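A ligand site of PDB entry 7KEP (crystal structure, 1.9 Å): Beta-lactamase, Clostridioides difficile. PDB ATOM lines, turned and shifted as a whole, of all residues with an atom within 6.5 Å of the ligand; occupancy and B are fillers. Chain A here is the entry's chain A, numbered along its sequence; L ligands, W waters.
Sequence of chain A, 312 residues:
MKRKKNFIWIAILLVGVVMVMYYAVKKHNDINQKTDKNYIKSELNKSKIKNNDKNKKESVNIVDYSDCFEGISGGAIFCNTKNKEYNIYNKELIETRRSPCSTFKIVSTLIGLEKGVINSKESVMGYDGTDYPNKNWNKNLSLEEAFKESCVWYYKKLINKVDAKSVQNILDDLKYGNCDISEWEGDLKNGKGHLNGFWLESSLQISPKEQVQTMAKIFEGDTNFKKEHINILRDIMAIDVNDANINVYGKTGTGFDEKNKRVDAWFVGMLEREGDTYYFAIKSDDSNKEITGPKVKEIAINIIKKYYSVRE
Merely in contact with the ligand: Cys 101 (3.5 Å), KCX 105 (3.4 Å), Val 152 (3.7 Å), Leu 200 (3.9 Å), Gly 253 (3.2 Å) and Pro 294 (3.7 Å). Hydrophobic or aromatic side chains within 4 Å of the ligand: Val 152, Leu 200 and Pro 294. Within 4 Å of the ligand: Cys 101, Ser 102, KCX 105, Ser 150, Val 152, Leu 200, Lys 251, Thr 252, Gly 253, Thr 254 and Pro 294.
The side-chain hydroxyl (OG) of Ser 102 sits at hydrogen-bond distance from the side-chain hydroxyl (OG) of Ser 150, 3.3 Å away. NZ of KCX 105 sits close to the side-chain hydroxyl of Ser 102, at 3.3 Å. The side-chain hydroxyl (OG) of Ser 150 sits at hydrogen-bond distance from the side-chain amino group (NZ) of Lys 251 (2.9 Å). The side-chain hydroxyl (OG1) of Thr 252 is in hydrogen-bond range of the side-chain amino group (NZ) of Lys 251 (3.4 Å). The backbone carbonyl oxygen of Gly 253 lies within hydrogen-bond range of the backbone NH of Trp 266, at 2.9 Å. SG of Cys 101 sits close to N of Gly 255. The side-chain sulfur (SG) of Cys 101 lies within hydrogen-bond range of the side-chain carboxylate (OE2) of Glu 201 (3.6 Å). The backbone NH (N) of Cys 101 sits at hydrogen-bond distance from the backbone carbonyl oxygen (O) of Trp 199, 2.9 Å away.
Water W1 lies within hydrogen-bond range of an oxygen (O2) of the ligand (2.8 Å), the backbone carbonyl oxygen of Leu 195 (2.9 Å) and the side-chain amino group of Lys 192 (3.3 Å).
N of Ser 102 is in hydrogen-bond range of O1 of the ligand (2.8 Å). C1 of the ligand is bonded to OG of Ser 102. O1 of the ligand sits at hydrogen-bond distance from N of Thr 254. The backbone carbonyl oxygen of Thr 254 is in hydrogen-bond range of a nitrogen (N2) of the ligand, 3.1 Å away. The side-chain hydroxyl (OG1) of Thr 254 lies within hydrogen-bond range of an oxygen (O6) of the ligand (2.5 Å). OG of Ser 150 sits at hydrogen-bond distance from N3 of the ligand, 2.8 Å away. The side-chain hydroxyl of Thr 252 lies within hydrogen-bond range of an oxygen (O5) of the ligand (2.8 Å). An oxygen (O5) of the ligand lies within salt-bridge range of the side-chain amino group (NZ) of Lys 251.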
ATOM      1  N   PRO A 100      -1.593 -11.837   3.948  1.00  0.00           N
ATOM      2  CA  PRO A 100      -2.617 -11.124   4.731  1.00  0.00           C
ATOM      3  C   PRO A 100      -2.322 -11.063   6.227  1.00  0.00           C
ATOM      4  O   PRO A 100      -2.931 -10.234   6.928  1.00  0.00           O
ATOM      5  CB  PRO A 100      -3.896 -11.937   4.462  1.00  0.00           C
ATOM      6  CG  PRO A 100      -3.412 -13.361   4.208  1.00  0.00           C
ATOM      7  CD  PRO A 100      -2.039 -13.190   3.532  1.00  0.00           C
ATOM      8  N   CYS A 101      -1.428 -11.911   6.742  1.00  0.00           N
ATOM      9  CA  CYS A 101      -1.205 -12.007   8.179  1.00  0.00           C
ATOM     10  C   CYS A 101      -2.542 -12.166   8.915  1.00  0.00           C
ATOM     11  O   CYS A 101      -3.424 -12.893   8.437  1.00  0.00           O
ATOM     12  CB  CYS A 101      -0.387 -10.810   8.677  1.00  0.00           C
ATOM     13  SG  CYS A 101       1.228 -10.719   7.769  1.00  0.00           S
ATOM     14  N   SER A 102      -2.711 -11.502  10.069  1.00  0.00           N
ATOM     15  CA  SER A 102      -3.924 -11.740  10.871  1.00  0.00           C
ATOM     16  C   SER A 102      -5.198 -11.239  10.237  1.00  0.00           C
ATOM     17  O   SER A 102      -6.269 -11.562  10.759  1.00  0.00           O
ATOM     18  CB  SER A 102      -3.806 -11.124  12.280  1.00  0.00           C
ATOM     19  OG  SER A 102      -2.723 -11.714  12.998  1.00  0.00           O
ATOM     20  N   THR A 103      -5.149 -10.446   9.158  1.00  0.00           N
ATOM     21  CA  THR A 103      -6.409 -10.133   8.477  1.00  0.00           C
ATOM     22  C   THR A 103      -7.092 -11.388   7.960  1.00  0.00           C
ATOM     23  O   THR A 103      -8.292 -11.355   7.659  1.00  0.00           O
ATOM     24  CB  THR A 103      -6.210  -9.126   7.325  1.00  0.00           C
ATOM     25  OG1 THR A 103      -5.457  -9.724   6.264  1.00  0.00           O
ATOM     26  CG2 THR A 103      -5.500  -7.863   7.808  1.00  0.00           C
ATOM     27  N   KCX A 105      -7.931 -13.814   9.599  1.00  0.00           N
ATOM     28  CA  KCX A 105      -8.901 -14.247  10.603  1.00  0.00           C
ATOM     29  CB  KCX A 105      -8.555 -13.626  11.965  1.00  0.00           C
ATOM     30  CG  KCX A 105      -7.272 -14.198  12.566  1.00  0.00           C
ATOM     31  CD  KCX A 105      -7.117 -13.720  14.039  1.00  0.00           C
ATOM     32  CE  KCX A 105      -5.963 -14.439  14.756  1.00  0.00           C
ATOM     33  NZ  KCX A 105      -4.599 -14.063  14.289  1.00  0.00           N
ATOM     34  C   KCX A 105     -10.351 -13.906  10.209  1.00  0.00           C
ATOM     35  O   KCX A 105     -11.310 -14.536  10.690  1.00  0.00           O
ATOM     36  CX  KCX A 105      -3.963 -14.723  13.294  1.00  0.00           C
ATOM     37  OQ1 KCX A 105      -4.485 -15.677  12.710  1.00  0.00           O
ATOM     38  OQ2 KCX A 105      -2.831 -14.383  12.933  1.00  0.00           O
ATOM     39  N   TRP A 137      -4.411 -14.772  26.145  1.00  0.00           N
ATOM     40  CA  TRP A 137      -4.391 -16.049  25.422  1.00  0.00           C
ATOM     41  C   TRP A 137      -4.417 -17.242  26.363  1.00  0.00           C
ATOM     42  O   TRP A 137      -4.584 -18.376  25.893  1.00  0.00           O
ATOM     43  CB  TRP A 137      -3.114 -16.162  24.583  1.00  0.00           C
ATOM     44  CG  TRP A 137      -3.000 -15.236  23.398  1.00  0.00           C
ATOM     45  CD1 TRP A 137      -3.689 -14.071  23.164  1.00  0.00           C
ATOM     46  CD2 TRP A 137      -2.066 -15.358  22.316  1.00  0.00           C
ATOM     47  NE1 TRP A 137      -3.283 -13.499  21.973  1.00  0.00           N
ATOM     48  CE2 TRP A 137      -2.265 -14.255  21.462  1.00  0.00           C
ATOM     49  CE3 TRP A 137      -1.095 -16.310  21.991  1.00  0.00           C
ATOM     50  CZ2 TRP A 137      -1.519 -14.074  20.292  1.00  0.00           C
ATOM     51  CZ3 TRP A 137      -0.354 -16.134  20.833  1.00  0.00           C
ATOM     52  CH2 TRP A 137      -0.575 -15.021  19.999  1.00  0.00           C
ATOM     53  N   GLU A 149      -8.420 -10.296  20.396  1.00  0.00           N
ATOM     54  CA  GLU A 149      -7.038 -10.455  20.846  1.00  0.00           C
ATOM     55  C   GLU A 149      -6.128 -11.023  19.768  1.00  0.00           C
ATOM     56  O   GLU A 149      -4.928 -11.220  20.034  1.00  0.00           O
ATOM     57  CB  GLU A 149      -6.971 -11.361  22.078  1.00  0.00           C
ATOM     58  CG  GLU A 149      -7.728 -10.793  23.256  1.00  0.00           C
ATOM     59  CD  GLU A 149      -6.907  -9.748  24.018  1.00  0.00           C
ATOM     60  OE1 GLU A 149      -5.708  -9.583  23.717  1.00  0.00           O
ATOM     61  OE2 GLU A 149      -7.498  -9.074  24.889  1.00  0.00           O
ATOM     62  N   SER A 150      -6.643 -11.305  18.584  1.00  0.00           N
ATOM     63  CA  SER A 150      -5.837 -11.840  17.503  1.00  0.00           C
ATOM     64  C   SER A 150      -5.085 -13.095  17.976  1.00  0.00           C
ATOM     65  O   SER A 150      -3.887 -13.248  17.740  1.00  0.00           O
ATOM     66  CB  SER A 150      -4.877 -10.754  16.997  1.00  0.00           C
ATOM     67  OG  SER A 150      -4.568 -10.914  15.632  1.00  0.00           O
ATOM     68  N   CYS A 151      -5.805 -13.980  18.682  1.00  0.00           N
ATOM     69  CA  CYS A 151      -5.176 -15.102  19.380  1.00  0.00           C
ATOM     70  C   CYS A 151      -4.782 -16.180  18.373  1.00  0.00           C
ATOM     71  O   CYS A 151      -5.640 -16.829  17.765  1.00  0.00           O
ATOM     72  CB  CYS A 151      -6.115 -15.650  20.455  1.00  0.00           C
ATOM     73  SG  CYS A 151      -5.552 -17.204  21.203  1.00  0.00           S
ATOM     74  N   VAL A 152      -3.477 -16.382  18.207  1.00  0.00           N
ATOM     75  CA  VAL A 152      -2.992 -17.245  17.144  1.00  0.00           C
ATOM     76  C   VAL A 152      -3.328 -18.712  17.422  1.00  0.00           C
ATOM     77  O   VAL A 152      -3.627 -19.466  16.495  1.00  0.00           O
ATOM     78  CB  VAL A 152      -1.490 -17.027  16.934  1.00  0.00           C
ATOM     79  CG1 VAL A 152      -0.948 -18.061  15.953  1.00  0.00           C
ATOM     80  CG2 VAL A 152      -1.249 -15.624  16.365  1.00  0.00           C
ATOM     81  N   LYS A 192       9.015 -20.152  15.263  1.00  0.00           N
ATOM     82  CA  LYS A 192       7.836 -20.064  16.114  1.00  0.00           C
ATOM     83  C   LYS A 192       6.957 -21.311  16.091  1.00  0.00           C
ATOM     84  O   LYS A 192       5.938 -21.343  16.776  1.00  0.00           O
ATOM     85  CB  LYS A 192       6.997 -18.837  15.734  1.00  0.00           C
ATOM     86  CG  LYS A 192       7.814 -17.540  15.801  1.00  0.00           C
ATOM     87  CD  LYS A 192       6.980 -16.311  15.392  1.00  0.00           C
ATOM     88  CE  LYS A 192       5.686 -16.229  16.146  1.00  0.00           C
ATOM     89  NZ  LYS A 192       5.204 -14.801  16.263  1.00  0.00           N
ATOM     90  N   LEU A 195       2.987 -21.589  16.077  1.00  0.00           N
ATOM     91  CA  LEU A 195       2.473 -20.218  15.931  1.00  0.00           C
ATOM     92  C   LEU A 195       2.773 -19.688  14.527  1.00  0.00           C
ATOM     93  O   LEU A 195       3.431 -18.674  14.327  1.00  0.00           O
ATOM     94  CB  LEU A 195       3.080 -19.308  17.001  1.00  0.00           C
ATOM     95  CG  LEU A 195       2.781 -19.715  18.448  1.00  0.00           C
ATOM     96  CD1 LEU A 195       3.607 -18.871  19.406  1.00  0.00           C
ATOM     97  CD2 LEU A 195       1.277 -19.496  18.689  1.00  0.00           C
ATOM     98  N   TRP A 199      -1.161 -18.415   6.163  1.00  0.00           N
ATOM     99  CA  TRP A 199      -1.601 -17.027   6.062  1.00  0.00           C
ATOM    100  C   TRP A 199      -0.669 -16.020   6.721  1.00  0.00           C
ATOM    101  O   TRP A 199      -0.944 -14.817   6.649  1.00  0.00           O
ATOM    102  CB  TRP A 199      -3.009 -16.901   6.675  1.00  0.00           C
ATOM    103  CG  TRP A 199      -3.017 -17.186   8.164  1.00  0.00           C
ATOM    104  CD1 TRP A 199      -2.971 -16.272   9.171  1.00  0.00           C
ATOM    105  CD2 TRP A 199      -3.069 -18.487   8.799  1.00  0.00           C
ATOM    106  NE1 TRP A 199      -2.991 -16.915  10.394  1.00  0.00           N
ATOM    107  CE2 TRP A 199      -3.059 -18.265  10.184  1.00  0.00           C
ATOM    108  CE3 TRP A 199      -3.152 -19.800   8.321  1.00  0.00           C
ATOM    109  CZ2 TRP A 199      -3.104 -19.317  11.110  1.00  0.00           C
ATOM    110  CZ3 TRP A 199      -3.185 -20.845   9.247  1.00  0.00           C
ATOM    111  CH2 TRP A 199      -3.166 -20.596  10.622  1.00  0.00           C
ATOM    112  N   LEU A 200       0.436 -16.460   7.355  1.00  0.00           N
ATOM    113  CA  LEU A 200       1.323 -15.591   8.136  1.00  0.00           C
ATOM    114  C   LEU A 200       2.713 -15.593   7.492  1.00  0.00           C
ATOM    115  O   LEU A 200       3.528 -16.488   7.763  1.00  0.00           O
ATOM    116  CB  LEU A 200       1.414 -16.051   9.600  1.00  0.00           C
ATOM    117  CG  LEU A 200       0.133 -15.985  10.458  1.00  0.00           C
ATOM    118  CD1 LEU A 200       0.186 -16.895  11.707  1.00  0.00           C
ATOM    119  CD2 LEU A 200      -0.263 -14.559  10.860  1.00  0.00           C
ATOM    120  N   GLU A 201       2.979 -14.585   6.651  1.00  0.00           N
ATOM    121  CA  GLU A 201       4.255 -14.445   5.931  1.00  0.00           C
ATOM    122  C   GLU A 201       4.701 -15.764   5.284  1.00  0.00           C
ATOM    123  O   GLU A 201       5.832 -16.218   5.451  1.00  0.00           O
ATOM    124  CB  GLU A 201       5.348 -13.890   6.852  1.00  0.00           C
ATOM    125  CG  GLU A 201       5.122 -12.442   7.280  1.00  0.00           C
ATOM    126  CD  GLU A 201       5.074 -11.466   6.107  1.00  0.00           C
ATOM    127  OE1 GLU A 201       5.640 -11.760   5.040  1.00  0.00           O
ATOM    128  OE2 GLU A 201       4.462 -10.406   6.276  1.00  0.00           O
ATOM    129  N   LYS A 251     -10.095  -5.437  10.850  1.00  0.00           N
ATOM    130  CA  LYS A 251      -9.117  -6.293  11.509  1.00  0.00           C
ATOM    131  C   LYS A 251      -7.714  -5.870  11.100  1.00  0.00           C
ATOM    132  O   LYS A 251      -7.449  -5.623   9.916  1.00  0.00           O
ATOM    133  CB  LYS A 251      -9.348  -7.777  11.139  1.00  0.00           C
ATOM    134  CG  LYS A 251      -8.323  -8.740  11.715  1.00  0.00           C
ATOM    135  CD  LYS A 251      -8.588  -9.038  13.203  1.00  0.00           C
ATOM    136  CE  LYS A 251      -7.422  -9.847  13.856  1.00  0.00           C
ATOM    137  NZ  LYS A 251      -6.175  -9.000  14.087  1.00  0.00           N
ATOM    138  N   THR A 252      -6.808  -5.792  12.070  1.00  0.00           N
ATOM    139  CA  THR A 252      -5.411  -5.513  11.811  1.00  0.00           C
ATOM    140  C   THR A 252      -4.637  -6.782  11.434  1.00  0.00           C
ATOM    141  O   THR A 252      -5.052  -7.916  11.727  1.00  0.00           O
ATOM    142  CB  THR A 252      -4.752  -4.908  13.053  1.00  0.00           C
ATOM    143  OG1 THR A 252      -4.918  -5.810  14.147  1.00  0.00           O
ATOM    144  CG2 THR A 252      -5.391  -3.562  13.408  1.00  0.00           C
ATOM    145  N   GLY A 253      -3.476  -6.570  10.845  1.00  0.00           N
ATOM    146  CA  GLY A 253      -2.521  -7.653  10.630  1.00  0.00           C
ATOM    147  C   GLY A 253      -1.119  -7.085  10.613  1.00  0.00           C
ATOM    148  O   GLY A 253      -0.900  -5.948  10.203  1.00  0.00           O
ATOM    149  N   THR A 254      -0.158  -7.881  11.094  1.00  0.00           N
ATOM    150  CA  THR A 254       1.228  -7.444  11.188  1.00  0.00           C
ATOM    151  C   THR A 254       2.147  -8.585  10.823  1.00  0.00           C
ATOM    152  O   THR A 254       2.047  -9.677  11.386  1.00  0.00           O
ATOM    153  CB  THR A 254       1.587  -6.963  12.612  1.00  0.00           C
ATOM    154  OG1 THR A 254       0.701  -5.927  13.028  1.00  0.00           O
ATOM    155  CG2 THR A 254       3.018  -6.442  12.611  1.00  0.00           C
ATOM    156  N   GLY A 255       3.058  -8.336   9.883  1.00  0.00           N
ATOM    157  CA  GLY A 255       4.089  -9.304   9.583  1.00  0.00           C
ATOM    158  C   GLY A 255       5.305  -8.567   9.066  1.00  0.00           C
ATOM    159  O   GLY A 255       5.263  -7.362   8.818  1.00  0.00           O
ATOM    160  N   PHE A 256       6.407  -9.304   8.912  1.00  0.00           N
ATOM    161  CA  PHE A 256       7.615  -8.720   8.347  1.00  0.00           C
ATOM    162  C   PHE A 256       8.035  -9.566   7.152  1.00  0.00           C
ATOM    163  O   PHE A 256       8.221 -10.784   7.272  1.00  0.00           O
ATOM    164  CB  PHE A 256       8.745  -8.626   9.378  1.00  0.00           C
ATOM    165  CG  PHE A 256       9.932  -7.828   8.884  1.00  0.00           C
ATOM    166  CD1 PHE A 256       9.864  -6.449   8.801  1.00  0.00           C
ATOM    167  CD2 PHE A 256      11.090  -8.468   8.474  1.00  0.00           C
ATOM    168  CE1 PHE A 256      10.957  -5.713   8.334  1.00  0.00           C
ATOM    169  CE2 PHE A 256      12.188  -7.740   7.997  1.00  0.00           C
ATOM    170  CZ  PHE A 256      12.106  -6.352   7.930  1.00  0.00           C
ATOM    171  N   TRP A 266      -1.421  -4.000   8.050  1.00  0.00           N
ATOM    172  CA  TRP A 266      -2.727  -3.961   7.409  1.00  0.00           C
ATOM    173  C   TRP A 266      -3.802  -3.415   8.349  1.00  0.00           C
ATOM    174  O   TRP A 266      -3.800  -3.705   9.539  1.00  0.00           O
ATOM    175  CB  TRP A 266      -3.224  -5.376   7.053  1.00  0.00           C
ATOM    176  CG  TRP A 266      -2.535  -6.166   6.011  1.00  0.00           C
ATOM    177  CD1 TRP A 266      -1.545  -7.093   6.206  1.00  0.00           C
ATOM    178  CD2 TRP A 266      -2.886  -6.238   4.618  1.00  0.00           C
ATOM    179  NE1 TRP A 266      -1.224  -7.697   5.006  1.00  0.00           N
ATOM    180  CE2 TRP A 266      -2.036  -7.184   4.029  1.00  0.00           C
ATOM    181  CE3 TRP A 266      -3.811  -5.558   3.820  1.00  0.00           C
ATOM    182  CZ2 TRP A 266      -2.086  -7.489   2.668  1.00  0.00           C
ATOM    183  CZ3 TRP A 266      -3.870  -5.862   2.464  1.00  0.00           C
ATOM    184  CH2 TRP A 266      -3.017  -6.824   1.901  1.00  0.00           C
ATOM    185  N   THR A 292       3.216  -1.174  12.600  1.00  0.00           N
ATOM    186  CA  THR A 292       2.453  -2.379  12.868  1.00  0.00           C
ATOM    187  C   THR A 292       1.041  -2.230  12.328  1.00  0.00           C
ATOM    188  O   THR A 292       0.614  -1.150  11.920  1.00  0.00           O
ATOM    189  CB  THR A 292       2.387  -2.662  14.375  1.00  0.00           C
ATOM    190  OG1 THR A 292       1.687  -1.579  15.021  1.00  0.00           O
ATOM    191  CG2 THR A 292       3.782  -2.781  14.960  1.00  0.00           C
ATOM    192  N   GLY A 293       0.289  -3.330  12.342  1.00  0.00           N
ATOM    193  CA  GLY A 293      -1.118  -3.270  12.061  1.00  0.00           C
ATOM    194  C   GLY A 293      -1.866  -2.210  12.867  1.00  0.00           C
ATOM    195  O   GLY A 293      -2.604  -1.402  12.307  1.00  0.00           O
ATOM    196  N   PRO A 294      -1.709  -2.190  14.194  1.00  0.00           N
ATOM    197  CA  PRO A 294      -2.388  -1.146  14.979  1.00  0.00           C
ATOM    198  C   PRO A 294      -2.025   0.270  14.577  1.00  0.00           C
ATOM    199  O   PRO A 294      -2.885   1.162  14.645  1.00  0.00           O
ATOM    200  CB  PRO A 294      -1.991  -1.458  16.428  1.00  0.00           C
ATOM    201  CG  PRO A 294      -1.653  -2.943  16.410  1.00  0.00           C
ATOM    202  CD  PRO A 294      -1.157  -3.274  15.032  1.00  0.00           C
HETATM  203  O1  LIG L   1      -1.089 -10.465  12.049  1.00  0.00           O
HETATM  204  C1  LIG L   1      -1.386 -11.315  12.895  1.00  0.00           C
HETATM  205  N1  LIG L   1      -0.663 -11.573  13.900  1.00  0.00           N
HETATM  206  C2  LIG L   1      -1.196 -12.193  15.120  1.00  0.00           C
HETATM  207  C3  LIG L   1       0.764 -11.249  13.882  1.00  0.00           C
HETATM  208  C4  LIG L   1       1.620 -12.466  13.697  1.00  0.00           C
HETATM  209  O2  LIG L   1       1.344 -13.516  14.233  1.00  0.00           O
HETATM  210  N2  LIG L   1       2.685 -12.338  12.898  1.00  0.00           N
HETATM  211  C5  LIG L   1       1.149 -10.508  15.154  1.00  0.00           C
HETATM  212  C6  LIG L   1       0.342 -10.785  16.431  1.00  0.00           C
HETATM  213  C7  LIG L   1      -1.124 -11.126  16.207  1.00  0.00           C
HETATM  214  N3  LIG L   1      -1.976  -9.944  15.893  1.00  0.00           N
HETATM  215  O3  LIG L   1      -1.325  -8.836  15.470  1.00  0.00           O
HETATM  216  S1  LIG L   1      -2.136  -7.638  14.927  1.00  0.00           S
HETATM  217  O4  LIG L   1      -2.425  -6.660  16.008  1.00  0.00           O
HETATM  218  O5  LIG L   1      -3.398  -8.180  14.409  1.00  0.00           O
HETATM  219  O6  LIG L   1      -1.460  -6.933  13.838  1.00  0.00           O
HETATM  220  O   HOH W   1       2.396 -16.004  14.962  1.00  0.00           O
